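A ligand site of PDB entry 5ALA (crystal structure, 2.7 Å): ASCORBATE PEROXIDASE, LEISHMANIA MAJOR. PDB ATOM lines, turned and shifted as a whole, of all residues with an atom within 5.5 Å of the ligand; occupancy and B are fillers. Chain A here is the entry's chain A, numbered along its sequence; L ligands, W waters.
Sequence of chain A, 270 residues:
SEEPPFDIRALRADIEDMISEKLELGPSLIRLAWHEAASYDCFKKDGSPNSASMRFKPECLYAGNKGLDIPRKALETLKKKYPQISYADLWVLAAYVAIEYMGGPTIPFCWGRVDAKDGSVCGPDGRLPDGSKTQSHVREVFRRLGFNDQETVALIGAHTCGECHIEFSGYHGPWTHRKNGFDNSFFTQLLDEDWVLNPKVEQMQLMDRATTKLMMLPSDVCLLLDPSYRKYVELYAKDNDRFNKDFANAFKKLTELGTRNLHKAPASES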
ATOM      1  N   GLU A  24     -15.966  -8.657 -21.091  1.00  0.00           N
ATOM      2  CA  GLU A  24     -16.441  -9.303 -19.889  1.00  0.00           C
ATOM      3  C   GLU A  24     -15.406 -10.286 -19.373  1.00  0.00           C
ATOM      4  O   GLU A  24     -15.576 -10.862 -18.312  1.00  0.00           O
ATOM      5  CB  GLU A  24     -17.772 -10.006 -20.139  1.00  0.00           C
ATOM      6  CG  GLU A  24     -17.828 -10.886 -21.374  1.00  0.00           C
ATOM      7  CD  GLU A  24     -18.147 -10.096 -22.644  1.00  0.00           C
ATOM      8  OE1 GLU A  24     -18.065  -8.851 -22.621  1.00  0.00           O
ATOM      9  OE2 GLU A  24     -18.522 -10.731 -23.656  1.00  0.00           O
ATOM     10  N   PRO A  27     -13.069  -8.368 -15.990  1.00  0.00           N
ATOM     11  CA  PRO A  27     -13.485  -8.589 -14.586  1.00  0.00           C
ATOM     12  C   PRO A  27     -13.331 -10.034 -14.170  1.00  0.00           C
ATOM     13  O   PRO A  27     -12.917 -10.339 -13.047  1.00  0.00           O
ATOM     14  CB  PRO A  27     -14.953  -8.178 -14.585  1.00  0.00           C
ATOM     15  CG  PRO A  27     -15.069  -7.206 -15.690  1.00  0.00           C
ATOM     16  CD  PRO A  27     -14.125  -7.684 -16.760  1.00  0.00           C
ATOM     17  N   SER A  28     -13.670 -10.927 -15.096  1.00  0.00           N
ATOM     18  CA  SER A  28     -13.581 -12.355 -14.842  1.00  0.00           C
ATOM     19  C   SER A  28     -12.135 -12.828 -14.579  1.00  0.00           C
ATOM     20  O   SER A  28     -11.913 -13.794 -13.845  1.00  0.00           O
ATOM     21  CB  SER A  28     -14.191 -13.097 -16.031  1.00  0.00           C
ATOM     22  OG  SER A  28     -13.667 -14.402 -16.184  1.00  0.00           O
ATOM     23  N   ILE A  30      -9.811 -10.934 -13.051  1.00  0.00           N
ATOM     24  CA  ILE A  30      -9.566 -10.535 -11.684  1.00  0.00           C
ATOM     25  C   ILE A  30     -10.122 -11.552 -10.682  1.00  0.00           C
ATOM     26  O   ILE A  30      -9.419 -11.968  -9.773  1.00  0.00           O
ATOM     27  CB  ILE A  30     -10.202  -9.167 -11.377  1.00  0.00           C
ATOM     28  CG1 ILE A  30      -9.601  -8.080 -12.247  1.00  0.00           C
ATOM     29  CG2 ILE A  30      -9.968  -8.766  -9.940  1.00  0.00           C
ATOM     30  CD1 ILE A  30     -10.195  -6.722 -11.898  1.00  0.00           C
ATOM     31  N   ARG A  31     -11.373 -11.977 -10.873  1.00  0.00           N
ATOM     32  CA  ARG A  31     -11.954 -12.951  -9.958  1.00  0.00           C
ATOM     33  C   ARG A  31     -11.122 -14.222  -9.901  1.00  0.00           C
ATOM     34  O   ARG A  31     -10.879 -14.767  -8.827  1.00  0.00           O
ATOM     35  CB  ARG A  31     -13.405 -13.272 -10.346  1.00  0.00           C
ATOM     36  CG  ARG A  31     -14.207 -14.081  -9.293  1.00  0.00           C
ATOM     37  CD  ARG A  31     -15.642 -14.428  -9.797  1.00  0.00           C
ATOM     38  NE  ARG A  31     -16.218 -15.561  -9.065  1.00  0.00           N
ATOM     39  CZ  ARG A  31     -16.977 -16.525  -9.597  1.00  0.00           C
ATOM     40  NH1 ARG A  31     -17.294 -16.511 -10.895  1.00  0.00           N
ATOM     41  NH2 ARG A  31     -17.419 -17.513  -8.832  1.00  0.00           N
ATOM     42  N   TRP A  34      -8.022 -13.977  -7.840  1.00  0.00           N
ATOM     43  CA  TRP A  34      -8.363 -13.687  -6.452  1.00  0.00           C
ATOM     44  C   TRP A  34      -8.880 -14.937  -5.723  1.00  0.00           C
ATOM     45  O   TRP A  34      -8.416 -15.232  -4.632  1.00  0.00           O
ATOM     46  CB  TRP A  34      -9.369 -12.511  -6.442  1.00  0.00           C
ATOM     47  CG  TRP A  34     -10.620 -12.601  -5.613  1.00  0.00           C
ATOM     48  CD1 TRP A  34     -11.906 -12.453  -6.064  1.00  0.00           C
ATOM     49  CD2 TRP A  34     -10.718 -12.794  -4.193  1.00  0.00           C
ATOM     50  NE1 TRP A  34     -12.798 -12.563  -5.022  1.00  0.00           N
ATOM     51  CE2 TRP A  34     -12.091 -12.778  -3.865  1.00  0.00           C
ATOM     52  CE3 TRP A  34      -9.783 -12.991  -3.181  1.00  0.00           C
ATOM     53  CZ2 TRP A  34     -12.542 -12.953  -2.563  1.00  0.00           C
ATOM     54  CZ3 TRP A  34     -10.241 -13.174  -1.889  1.00  0.00           C
ATOM     55  CH2 TRP A  34     -11.608 -13.146  -1.587  1.00  0.00           C
ATOM     56  N   HIS A  35      -9.755 -15.708  -6.333  1.00  0.00           N
ATOM     57  CA  HIS A  35     -10.212 -16.914  -5.674  1.00  0.00           C
ATOM     58  C   HIS A  35      -9.143 -17.990  -5.647  1.00  0.00           C
ATOM     59  O   HIS A  35      -9.209 -18.908  -4.836  1.00  0.00           O
ATOM     60  CB  HIS A  35     -11.490 -17.453  -6.302  1.00  0.00           C
ATOM     61  CG  HIS A  35     -12.721 -16.750  -5.829  1.00  0.00           C
ATOM     62  ND1 HIS A  35     -13.994 -17.215  -6.086  1.00  0.00           N
ATOM     63  CD2 HIS A  35     -12.876 -15.614  -5.101  1.00  0.00           C
ATOM     64  CE1 HIS A  35     -14.874 -16.381  -5.550  1.00  0.00           C
ATOM     65  NE2 HIS A  35     -14.220 -15.406  -4.942  1.00  0.00           N
ATOM     66  N   PRO A 129     -15.567 -16.527   0.676  1.00  0.00           N
ATOM     67  CA  PRO A 129     -16.608 -15.748   1.365  1.00  0.00           C
ATOM     68  C   PRO A 129     -18.035 -15.883   0.785  1.00  0.00           C
ATOM     69  O   PRO A 129     -18.201 -16.033  -0.454  1.00  0.00           O
ATOM     70  CB  PRO A 129     -16.108 -14.307   1.217  1.00  0.00           C
ATOM     71  CG  PRO A 129     -15.250 -14.308   0.041  1.00  0.00           C
ATOM     72  CD  PRO A 129     -14.603 -15.658  -0.009  1.00  0.00           C
ATOM     73  N   ASP A 130     -19.041 -15.737   1.648  1.00  0.00           N
ATOM     74  CA  ASP A 130     -20.439 -15.859   1.248  1.00  0.00           C
ATOM     75  C   ASP A 130     -21.123 -14.481   1.193  1.00  0.00           C
ATOM     76  O   ASP A 130     -21.321 -13.846   2.226  1.00  0.00           O
ATOM     77  CB  ASP A 130     -21.169 -16.777   2.230  1.00  0.00           C
ATOM     78  CG  ASP A 130     -22.541 -17.201   1.728  1.00  0.00           C
ATOM     79  OD1 ASP A 130     -23.167 -16.480   0.909  1.00  0.00           O
ATOM     80  OD2 ASP A 130     -23.002 -18.280   2.191  1.00  0.00           O
ATOM     81  N   GLY A 131     -21.531 -14.056  -0.010  1.00  0.00           N
ATOM     82  CA  GLY A 131     -22.160 -12.753  -0.230  1.00  0.00           C
ATOM     83  C   GLY A 131     -23.477 -12.584   0.522  1.00  0.00           C
ATOM     84  O   GLY A 131     -23.942 -11.453   0.725  1.00  0.00           O
ATOM     85  N   VAL A 138     -17.239 -11.433   6.878  1.00  0.00           N
ATOM     86  CA  VAL A 138     -16.234 -10.793   6.044  1.00  0.00           C
ATOM     87  C   VAL A 138     -14.939 -10.621   6.836  1.00  0.00           C
ATOM     88  O   VAL A 138     -13.869 -11.050   6.394  1.00  0.00           O
ATOM     89  CB  VAL A 138     -16.698  -9.409   5.538  1.00  0.00           C
ATOM     90  CG1 VAL A 138     -15.512  -8.660   4.908  1.00  0.00           C
ATOM     91  CG2 VAL A 138     -17.899  -9.559   4.585  1.00  0.00           C
ATOM     92  N   PHE A 142     -11.125 -12.267   5.743  1.00  0.00           N
ATOM     93  CA  PHE A 142      -9.945 -11.460   5.451  1.00  0.00           C
ATOM     94  C   PHE A 142      -8.890 -11.479   6.562  1.00  0.00           C
ATOM     95  O   PHE A 142      -7.720 -11.230   6.292  1.00  0.00           O
ATOM     96  CB  PHE A 142     -10.372 -10.025   5.152  1.00  0.00           C
ATOM     97  CG  PHE A 142     -10.841  -9.832   3.760  1.00  0.00           C
ATOM     98  CD1 PHE A 142     -12.075 -10.335   3.368  1.00  0.00           C
ATOM     99  CD2 PHE A 142     -10.056  -9.179   2.824  1.00  0.00           C
ATOM    100  CE1 PHE A 142     -12.520 -10.186   2.063  1.00  0.00           C
ATOM    101  CE2 PHE A 142     -10.496  -9.009   1.507  1.00  0.00           C
ATOM    102  CZ  PHE A 142     -11.716  -9.513   1.118  1.00  0.00           C
ATOM    103  N   LEU A 155      -9.736  -4.287  -1.372  1.00  0.00           N
ATOM    104  CA  LEU A 155      -9.860  -5.438  -2.252  1.00  0.00           C
ATOM    105  C   LEU A 155     -11.271  -5.621  -2.791  1.00  0.00           C
ATOM    106  O   LEU A 155     -11.441  -6.004  -3.948  1.00  0.00           O
ATOM    107  CB  LEU A 155      -9.399  -6.704  -1.560  1.00  0.00           C
ATOM    108  CG  LEU A 155      -7.879  -6.838  -1.470  1.00  0.00           C
ATOM    109  CD1 LEU A 155      -7.484  -7.981  -0.508  1.00  0.00           C
ATOM    110  CD2 LEU A 155      -7.314  -7.076  -2.870  1.00  0.00           C
ATOM    111  N   ILE A 156     -12.277  -5.400  -1.963  1.00  0.00           N
ATOM    112  CA  ILE A 156     -13.659  -5.577  -2.410  1.00  0.00           C
ATOM    113  C   ILE A 156     -14.046  -4.463  -3.395  1.00  0.00           C
ATOM    114  O   ILE A 156     -14.997  -4.629  -4.168  1.00  0.00           O
ATOM    115  CB  ILE A 156     -14.629  -5.631  -1.201  1.00  0.00           C
ATOM    116  CG1 ILE A 156     -14.378  -6.913  -0.389  1.00  0.00           C
ATOM    117  CG2 ILE A 156     -16.084  -5.647  -1.665  1.00  0.00           C
ATOM    118  CD1 ILE A 156     -14.945  -6.887   1.009  1.00  0.00           C
ATOM    119  N   ALA A 158     -12.907  -3.985  -6.065  1.00  0.00           N
ATOM    120  CA  ALA A 158     -12.884  -4.608  -7.380  1.00  0.00           C
ATOM    121  C   ALA A 158     -14.283  -4.883  -7.921  1.00  0.00           C
ATOM    122  O   ALA A 158     -14.449  -5.169  -9.124  1.00  0.00           O
ATOM    123  CB  ALA A 158     -12.100  -5.882  -7.339  1.00  0.00           C
ATOM    124  N   HIS A 159     -15.307  -4.803  -7.083  1.00  0.00           N
ATOM    125  CA  HIS A 159     -16.677  -4.988  -7.564  1.00  0.00           C
ATOM    126  C   HIS A 159     -17.123  -3.745  -8.321  1.00  0.00           C
ATOM    127  O   HIS A 159     -18.254  -3.669  -8.796  1.00  0.00           O
ATOM    128  CB  HIS A 159     -17.631  -5.298  -6.417  1.00  0.00           C
ATOM    129  CG  HIS A 159     -17.491  -6.696  -5.883  1.00  0.00           C
ATOM    130  ND1 HIS A 159     -18.188  -7.148  -4.772  1.00  0.00           N
ATOM    131  CD2 HIS A 159     -16.754  -7.743  -6.310  1.00  0.00           C
ATOM    132  CE1 HIS A 159     -17.873  -8.411  -4.546  1.00  0.00           C
ATOM    133  NE2 HIS A 159     -17.002  -8.801  -5.460  1.00  0.00           N
ATOM    134  N   CYS A 161     -16.053  -3.323 -11.053  1.00  0.00           N
ATOM    135  CA  CYS A 161     -16.123  -3.863 -12.398  1.00  0.00           C
ATOM    136  C   CYS A 161     -16.732  -5.242 -12.335  1.00  0.00           C
ATOM    137  O   CYS A 161     -16.669  -5.906 -11.307  1.00  0.00           O
ATOM    138  CB  CYS A 161     -14.745  -3.905 -13.082  1.00  0.00           C
ATOM    139  SG  CYS A 161     -13.637  -5.190 -12.478  1.00  0.00           S
ATOM    140  N   GLY A 162     -17.337  -5.672 -13.430  1.00  0.00           N
ATOM    141  CA  GLY A 162     -17.954  -6.974 -13.483  1.00  0.00           C
ATOM    142  C   GLY A 162     -19.402  -6.974 -13.054  1.00  0.00           C
ATOM    143  O   GLY A 162     -20.022  -5.925 -12.809  1.00  0.00           O
ATOM    144  N   GLU A 163     -19.945  -8.180 -12.967  1.00  0.00           N
ATOM    145  CA  GLU A 163     -21.347  -8.363 -12.645  1.00  0.00           C
ATOM    146  C   GLU A 163     -21.564  -9.780 -12.098  1.00  0.00           C
ATOM    147  O   GLU A 163     -20.702 -10.642 -12.242  1.00  0.00           O
ATOM    148  CB  GLU A 163     -22.188  -8.124 -13.889  1.00  0.00           C
ATOM    149  CG  GLU A 163     -21.740  -8.969 -15.052  1.00  0.00           C
ATOM    150  CD  GLU A 163     -22.298  -8.542 -16.397  1.00  0.00           C
ATOM    151  OE1 GLU A 163     -23.238  -7.726 -16.466  1.00  0.00           O
ATOM    152  OE2 GLU A 163     -21.759  -9.019 -17.416  1.00  0.00           O
ATOM    153  N   CYS A 164     -22.716  -9.994 -11.474  1.00  0.00           N
ATOM    154  CA  CYS A 164     -23.114 -11.315 -10.991  1.00  0.00           C
ATOM    155  C   CYS A 164     -23.984 -12.022 -12.027  1.00  0.00           C
ATOM    156  O   CYS A 164     -24.752 -11.383 -12.736  1.00  0.00           O
ATOM    157  CB  CYS A 164     -23.883 -11.177  -9.690  1.00  0.00           C
ATOM    158  SG  CYS A 164     -22.964 -10.346  -8.393  1.00  0.00           S
ATOM    159  N   HIS A 165     -23.877 -13.347 -12.112  1.00  0.00           N
ATOM    160  CA  HIS A 165     -24.653 -14.091 -13.085  1.00  0.00           C
ATOM    161  C   HIS A 165     -25.412 -15.187 -12.353  1.00  0.00           C
ATOM    162  O   HIS A 165     -24.797 -16.001 -11.669  1.00  0.00           O
ATOM    163  CB  HIS A 165     -23.751 -14.696 -14.162  1.00  0.00           C
ATOM    164  CG  HIS A 165     -22.716 -13.743 -14.695  1.00  0.00           C
ATOM    165  ND1 HIS A 165     -21.419 -13.712 -14.230  1.00  0.00           N
ATOM    166  CD2 HIS A 165     -22.797 -12.775 -15.628  1.00  0.00           C
ATOM    167  CE1 HIS A 165     -20.753 -12.763 -14.851  1.00  0.00           C
ATOM    168  NE2 HIS A 165     -21.562 -12.183 -15.703  1.00  0.00           N
ATOM    169  N   ILE A 166     -26.749 -15.216 -12.493  1.00  0.00           N
ATOM    170  CA  ILE A 166     -27.609 -16.176 -11.799  1.00  0.00           C
ATOM    171  C   ILE A 166     -27.043 -17.576 -11.876  1.00  0.00           C
ATOM    172  O   ILE A 166     -26.977 -18.267 -10.879  1.00  0.00           O
ATOM    173  CB  ILE A 166     -29.050 -16.221 -12.364  1.00  0.00           C
ATOM    174  CG1 ILE A 166     -29.793 -14.890 -12.175  1.00  0.00           C
ATOM    175  CG2 ILE A 166     -29.864 -17.301 -11.640  1.00  0.00           C
ATOM    176  CD1 ILE A 166     -30.402 -14.694 -10.802  1.00  0.00           C
ATOM    177  N   PHE A 168     -24.205 -18.671 -12.049  1.00  0.00           N
ATOM    178  CA  PHE A 168     -22.912 -18.827 -11.381  1.00  0.00           C
ATOM    179  C   PHE A 168     -23.043 -18.735  -9.869  1.00  0.00           C
ATOM    180  O   PHE A 168     -22.700 -19.651  -9.137  1.00  0.00           O
ATOM    181  CB  PHE A 168     -21.923 -17.742 -11.806  1.00  0.00           C
ATOM    182  CG  PHE A 168     -21.419 -17.873 -13.205  1.00  0.00           C
ATOM    183  CD1 PHE A 168     -21.540 -19.058 -13.907  1.00  0.00           C
ATOM    184  CD2 PHE A 168     -20.815 -16.787 -13.829  1.00  0.00           C
ATOM    185  CE1 PHE A 168     -21.071 -19.159 -15.201  1.00  0.00           C
ATOM    186  CE2 PHE A 168     -20.341 -16.889 -15.114  1.00  0.00           C
ATOM    187  CZ  PHE A 168     -20.467 -18.077 -15.789  1.00  0.00           C
ATOM    188  N   SER A 169     -23.553 -17.603  -9.400  1.00  0.00           N
ATOM    189  CA  SER A 169     -23.554 -17.329  -7.983  1.00  0.00           C
ATOM    190  C   SER A 169     -24.974 -17.282  -7.392  1.00  0.00           C
ATOM    191  O   SER A 169     -25.142 -17.343  -6.157  1.00  0.00           O
ATOM    192  CB  SER A 169     -22.834 -16.014  -7.715  1.00  0.00           C
ATOM    193  OG  SER A 169     -23.529 -14.941  -8.305  1.00  0.00           O
ATOM    194  N   GLY A 170     -25.982 -17.179  -8.247  1.00  0.00           N
ATOM    195  CA  GLY A 170     -27.343 -17.060  -7.782  1.00  0.00           C
ATOM    196  C   GLY A 170     -27.751 -15.600  -7.656  1.00  0.00           C
ATOM    197  O   GLY A 170     -28.922 -15.272  -7.460  1.00  0.00           O
ATOM    198  N   TYR A 171     -26.771 -14.710  -7.729  1.00  0.00           N
ATOM    199  CA  TYR A 171     -27.032 -13.284  -7.689  1.00  0.00           C
ATOM    200  C   TYR A 171     -27.073 -12.752  -9.119  1.00  0.00           C
ATOM    201  O   TYR A 171     -26.872 -13.509 -10.077  1.00  0.00           O
ATOM    202  CB  TYR A 171     -25.980 -12.579  -6.845  1.00  0.00           C
ATOM    203  CG  TYR A 171     -25.981 -13.009  -5.390  1.00  0.00           C
ATOM    204  CD1 TYR A 171     -26.985 -12.590  -4.525  1.00  0.00           C
ATOM    205  CD2 TYR A 171     -25.008 -13.863  -4.893  1.00  0.00           C
ATOM    206  CE1 TYR A 171     -26.995 -12.971  -3.204  1.00  0.00           C
ATOM    207  CE2 TYR A 171     -25.005 -14.255  -3.570  1.00  0.00           C
ATOM    208  CZ  TYR A 171     -26.014 -13.802  -2.732  1.00  0.00           C
ATOM    209  OH  TYR A 171     -26.052 -14.180  -1.415  1.00  0.00           O
ATOM    210  N   TRP A 175     -22.518  -3.984 -10.321  1.00  0.00           N
ATOM    211  CA  TRP A 175     -22.478  -3.094  -9.160  1.00  0.00           C
ATOM    212  C   TRP A 175     -22.504  -1.624  -9.550  1.00  0.00           C
ATOM    213  O   TRP A 175     -22.906  -0.777  -8.754  1.00  0.00           O
ATOM    214  CB  TRP A 175     -21.229  -3.371  -8.311  1.00  0.00           C
ATOM    215  CG  TRP A 175     -21.269  -4.675  -7.582  1.00  0.00           C
ATOM    216  CD1 TRP A 175     -21.701  -4.867  -6.322  1.00  0.00           C
ATOM    217  CD2 TRP A 175     -20.806  -5.955  -8.046  1.00  0.00           C
ATOM    218  NE1 TRP A 175     -21.586  -6.188  -5.978  1.00  0.00           N
ATOM    219  CE2 TRP A 175     -21.038  -6.875  -7.020  1.00  0.00           C
ATOM    220  CE3 TRP A 175     -20.234  -6.402  -9.244  1.00  0.00           C
ATOM    221  CZ2 TRP A 175     -20.715  -8.238  -7.129  1.00  0.00           C
ATOM    222  CZ3 TRP A 175     -19.911  -7.765  -9.353  1.00  0.00           C
ATOM    223  CH2 TRP A 175     -20.151  -8.657  -8.303  1.00  0.00           C
ATOM    224  N   LEU A 217     -24.684  -6.739  -2.806  1.00  0.00           N
ATOM    225  CA  LEU A 217     -24.791  -7.928  -1.982  1.00  0.00           C
ATOM    226  C   LEU A 217     -24.917  -7.547  -0.517  1.00  0.00           C
ATOM    227  O   LEU A 217     -24.527  -6.437  -0.143  1.00  0.00           O
ATOM    228  CB  LEU A 217     -23.558  -8.829  -2.173  1.00  0.00           C
ATOM    229  CG  LEU A 217     -23.357  -9.474  -3.532  1.00  0.00           C
ATOM    230  CD1 LEU A 217     -22.017 -10.167  -3.609  1.00  0.00           C
ATOM    231  CD2 LEU A 217     -24.461 -10.515  -3.685  1.00  0.00           C
ATOM    232  N   SER A 219     -22.971  -8.841   1.600  1.00  0.00           N
ATOM    233  CA  SER A 219     -21.543  -8.665   1.940  1.00  0.00           C
ATOM    234  C   SER A 219     -20.988  -7.326   1.436  1.00  0.00           C
ATOM    235  O   SER A 219     -20.092  -6.759   2.042  1.00  0.00           O
ATOM    236  CB  SER A 219     -20.701  -9.815   1.369  1.00  0.00           C
ATOM    237  OG  SER A 219     -20.815  -9.887  -0.039  1.00  0.00           O
ATOM    238  N   PHE A 247      -5.441  -0.543  -3.629  1.00  0.00           N
ATOM    239  CA  PHE A 247      -5.865  -1.763  -4.310  1.00  0.00           C
ATOM    240  C   PHE A 247      -4.686  -2.493  -4.925  1.00  0.00           C
ATOM    241  O   PHE A 247      -4.594  -3.725  -4.858  1.00  0.00           O
ATOM    242  CB  PHE A 247      -6.910  -1.486  -5.390  1.00  0.00           C
ATOM    243  CG  PHE A 247      -7.402  -2.734  -6.029  1.00  0.00           C
ATOM    244  CD1 PHE A 247      -8.351  -3.519  -5.375  1.00  0.00           C
ATOM    245  CD2 PHE A 247      -6.857  -3.201  -7.212  1.00  0.00           C
ATOM    246  CE1 PHE A 247      -8.787  -4.704  -5.917  1.00  0.00           C
ATOM    247  CE2 PHE A 247      -7.286  -4.397  -7.761  1.00  0.00           C
ATOM    248  CZ  PHE A 247      -8.254  -5.150  -7.100  1.00  0.00           C
ATOM    249  N   PHE A 251      -3.765  -6.133  -3.743  1.00  0.00           N
ATOM    250  CA  PHE A 251      -3.959  -7.197  -4.706  1.00  0.00           C
ATOM    251  C   PHE A 251      -2.613  -7.860  -5.017  1.00  0.00           C
ATOM    252  O   PHE A 251      -2.543  -9.074  -5.241  1.00  0.00           O
ATOM    253  CB  PHE A 251      -4.625  -6.667  -5.979  1.00  0.00           C
ATOM    254  CG  PHE A 251      -5.144  -7.750  -6.864  1.00  0.00           C
ATOM    255  CD1 PHE A 251      -6.334  -8.385  -6.569  1.00  0.00           C
ATOM    256  CD2 PHE A 251      -4.425  -8.172  -7.975  1.00  0.00           C
ATOM    257  CE1 PHE A 251      -6.819  -9.403  -7.354  1.00  0.00           C
ATOM    258  CE2 PHE A 251      -4.897  -9.201  -8.760  1.00  0.00           C
ATOM    259  CZ  PHE A 251      -6.109  -9.816  -8.444  1.00  0.00           C
ATOM    260  N   LEU A 254      -2.006  -9.948  -1.897  1.00  0.00           N
ATOM    261  CA  LEU A 254      -2.910 -11.072  -2.097  1.00  0.00           C
ATOM    262  C   LEU A 254      -2.356 -12.127  -3.040  1.00  0.00           C
ATOM    263  O   LEU A 254      -2.282 -13.312  -2.704  1.00  0.00           O
ATOM    264  CB  LEU A 254      -4.238 -10.586  -2.626  1.00  0.00           C
ATOM    265  CG  LEU A 254      -5.172 -11.682  -3.109  1.00  0.00           C
ATOM    266  CD1 LEU A 254      -5.603 -12.602  -2.017  1.00  0.00           C
ATOM    267  CD2 LEU A 254      -6.371 -11.005  -3.717  1.00  0.00           C
HETATM  268  C1  LIG L   1     -18.001 -11.499  -8.800  1.00  0.00           C
HETATM  269  C2  LIG L   1     -18.905 -12.098  -4.013  1.00  0.00           C
HETATM  270  C3  LIG L   1     -14.657  -9.994  -2.849  1.00  0.00           C
HETATM  271  C4  LIG L   1     -13.683  -9.543  -7.553  1.00  0.00           C
HETATM  272  C5  LIG L   1     -18.623 -11.848  -7.599  1.00  0.00           C
HETATM  273  C6  LIG L   1     -19.900 -12.507  -7.444  1.00  0.00           C
HETATM  274  C7  LIG L   1     -20.144 -12.673  -6.126  1.00  0.00           C
HETATM  275  C8  LIG L   1     -19.042 -12.122  -5.384  1.00  0.00           C
HETATM  276  C9  LIG L   1     -21.396 -13.328  -5.469  1.00  0.00           C
HETATM  277  C10 LIG L   1     -20.797 -12.952  -8.608  1.00  0.00           C
HETATM  278  C11 LIG L   1     -20.129 -14.071  -9.372  1.00  0.00           C
HETATM  279  C12 LIG L   1     -20.888 -14.362 -10.652  1.00  0.00           C
HETATM  280  O1  LIG L   1     -21.951 -15.021 -10.576  1.00  0.00           O
HETATM  281  O2  LIG L   1     -20.412 -13.932 -11.748  1.00  0.00           O
HETATM  282  C13 LIG L   1     -17.833 -11.592  -3.296  1.00  0.00           C
HETATM  283  C14 LIG L   1     -17.702 -11.568  -1.847  1.00  0.00           C
HETATM  284  C15 LIG L   1     -16.526 -10.999  -1.538  1.00  0.00           C
HETATM  285  C16 LIG L   1     -15.882 -10.627  -2.776  1.00  0.00           C
HETATM  286  C17 LIG L   1     -18.752 -12.141  -0.869  1.00  0.00           C
HETATM  287  C18 LIG L   1     -15.858 -10.699  -0.179  1.00  0.00           C
HETATM  288  C19 LIG L   1     -16.438 -10.898   1.011  1.00  0.00           C
HETATM  289  C20 LIG L   1     -13.968  -9.766  -4.023  1.00  0.00           C
HETATM  290  C21 LIG L   1     -12.584  -9.385  -4.145  1.00  0.00           C
HETATM  291  C22 LIG L   1     -12.318  -9.291  -5.468  1.00  0.00           C
HETATM  292  C23 LIG L   1     -13.538  -9.580  -6.187  1.00  0.00           C
HETATM  293  C24 LIG L   1     -11.613  -9.194  -2.947  1.00  0.00           C
HETATM  294  C25 LIG L   1     -11.010  -8.902  -6.217  1.00  0.00           C
HETATM  295  C26 LIG L   1     -10.053  -8.150  -5.681  1.00  0.00           C
HETATM  296  C27 LIG L   1     -14.781  -9.880  -8.306  1.00  0.00           C
HETATM  297  C28 LIG L   1     -14.954  -9.503  -9.697  1.00  0.00           C
HETATM  298  C29 LIG L   1     -16.283 -10.114 -10.117  1.00  0.00           C
HETATM  299  C30 LIG L   1     -16.809 -10.794  -8.935  1.00  0.00           C
HETATM  300  C31 LIG L   1     -13.993  -8.681 -10.575  1.00  0.00           C
HETATM  301  C32 LIG L   1     -16.876  -9.969 -11.529  1.00  0.00           C
HETATM  302  C33 LIG L   1     -16.699 -11.304 -12.224  1.00  0.00           C
HETATM  303  C34 LIG L   1     -17.431 -11.219 -13.537  1.00  0.00           C
HETATM  304  O3  LIG L   1     -18.070 -10.147 -13.770  1.00  0.00           O
HETATM  305  O4  LIG L   1     -17.367 -12.195 -14.343  1.00  0.00           O
HETATM  306  N1  LIG L   1     -18.132 -11.633  -6.317  1.00  0.00           N
HETATM  307  N2  LIG L   1     -16.697 -11.004  -3.823  1.00  0.00           N
HETATM  308  N3  LIG L   1     -14.523  -9.868  -5.275  1.00  0.00           N
HETATM  309  N4  LIG L   1     -15.895 -10.629  -7.887  1.00  0.00           N
HETATM  310 FE1  LIG L   1     -16.379 -10.681  -5.783  1.00  0.00          FE
HETATM  311  O   HOH W   1     -15.886 -12.762  -6.028  1.00  0.00           O
HETATM  312  O   HOH W   2     -15.749 -14.033  -3.161  1.00  0.00           O
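The backbone NH (N) of Ser 169 lies close to an oxygen (O1) of the ligand, 3.3 Å away. An iron atom (FE1) of the ligand is bound by a ring nitrogen (NE2) of His 159, 2.0 Å away. The backbone carbonyl oxygen of Glu 163 sits close to an oxygen (O3) of the ligand (3.1 Å). The side-chain hydroxyl of Ser 169 sits at hydrogen-bond distance from an oxygen (O1) of the ligand (2.8 Å). N of His 165 is in hydrogen-bond range of O1 of the ligand (3.0 Å). The backbone NH (N) of Glu 163 lies within hydrogen-bond range of an oxygen (O3) of the ligand (2.8 Å). An oxygen (O2) of the ligand sits at hydrogen-bond distance from a ring nitrogen (ND1) of His 165, at 2.7 Å.
The indole nitrogen (NE1) of Trp 34 lies close to a ring nitrogen (NE2) of His 35. The backbone NH of Ile 166 sits at hydrogen-bond distance from the backbone carbonyl oxygen of Tyr 171, 3.0 Å away. O of Ala 158 is in hydrogen-bond range of SG of Cys 161 (3.5 Å). The side-chain hydroxyl of Ser 169 sits close to the backbone NH of Tyr 171 (3.3 Å). The backbone carbonyl oxygen (O) of Gly 131 is in hydrogen-bond range of the backbone NH (N) of Ser 219, at 2.9 Å.
N3 of the ligand sits close to NE1 of Trp 34 (3.2 Å). Merely in contact with the ligand: Pro 27 (3.2 Å), Ser 28 (3.7 Å), Ile 30 (3.9 Å), Arg 31 (3.9 Å), Pro 129 (3.4 Å), Asp 130 (3.9 Å), Gly 131 (3.5 Å), Leu 155 (3.1 Å), Ile 156 (3.95 Å), Ala 158 (3.4 Å), Cys 161 (3.9 Å), Gly 162 (3.2 Å), Cys 164 (3.4 Å), Phe 168 (3.0 Å), Tyr 171 (3.7 Å), Trp 175 (3.6 Å), Leu 217 (3.7 Å), Ser 219 (3.2 Å), Phe 247 (3.7 Å) and Phe 251 (3.8 Å). Hydrophobic or aromatic side chains within 4 Å of the ligand: Pro 27, Ile 30, Trp 34, Pro 129, Leu 155, Ile 156, Ala 158, His 159, His 165, Phe 168, Tyr 171, Trp 175, Leu 217, Phe 247 and Phe 251. Within 4 Å of the ligand: Pro 27, Ser 28, Ile 30, Arg 31, Trp 34, Pro 129, Asp 130, Gly 131, Leu 155, Ile 156, Ala 158, His 159, Cys 161, Gly 162, Glu 163, Cys 164, His 165, Phe 168, Ser 169, Tyr 171, Trp 175, Leu 217, Ser 219, Phe 247 and Phe 251. Along chain A the residues within 4 Å of the ligand span positions 27 to 251. The nearest printed residue that does not touch the ligand is Phe 142 (4.1 Å).
Water W1 bridges the indole nitrogen of Trp 34 and a ring nitrogen (NE2) of His 35.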
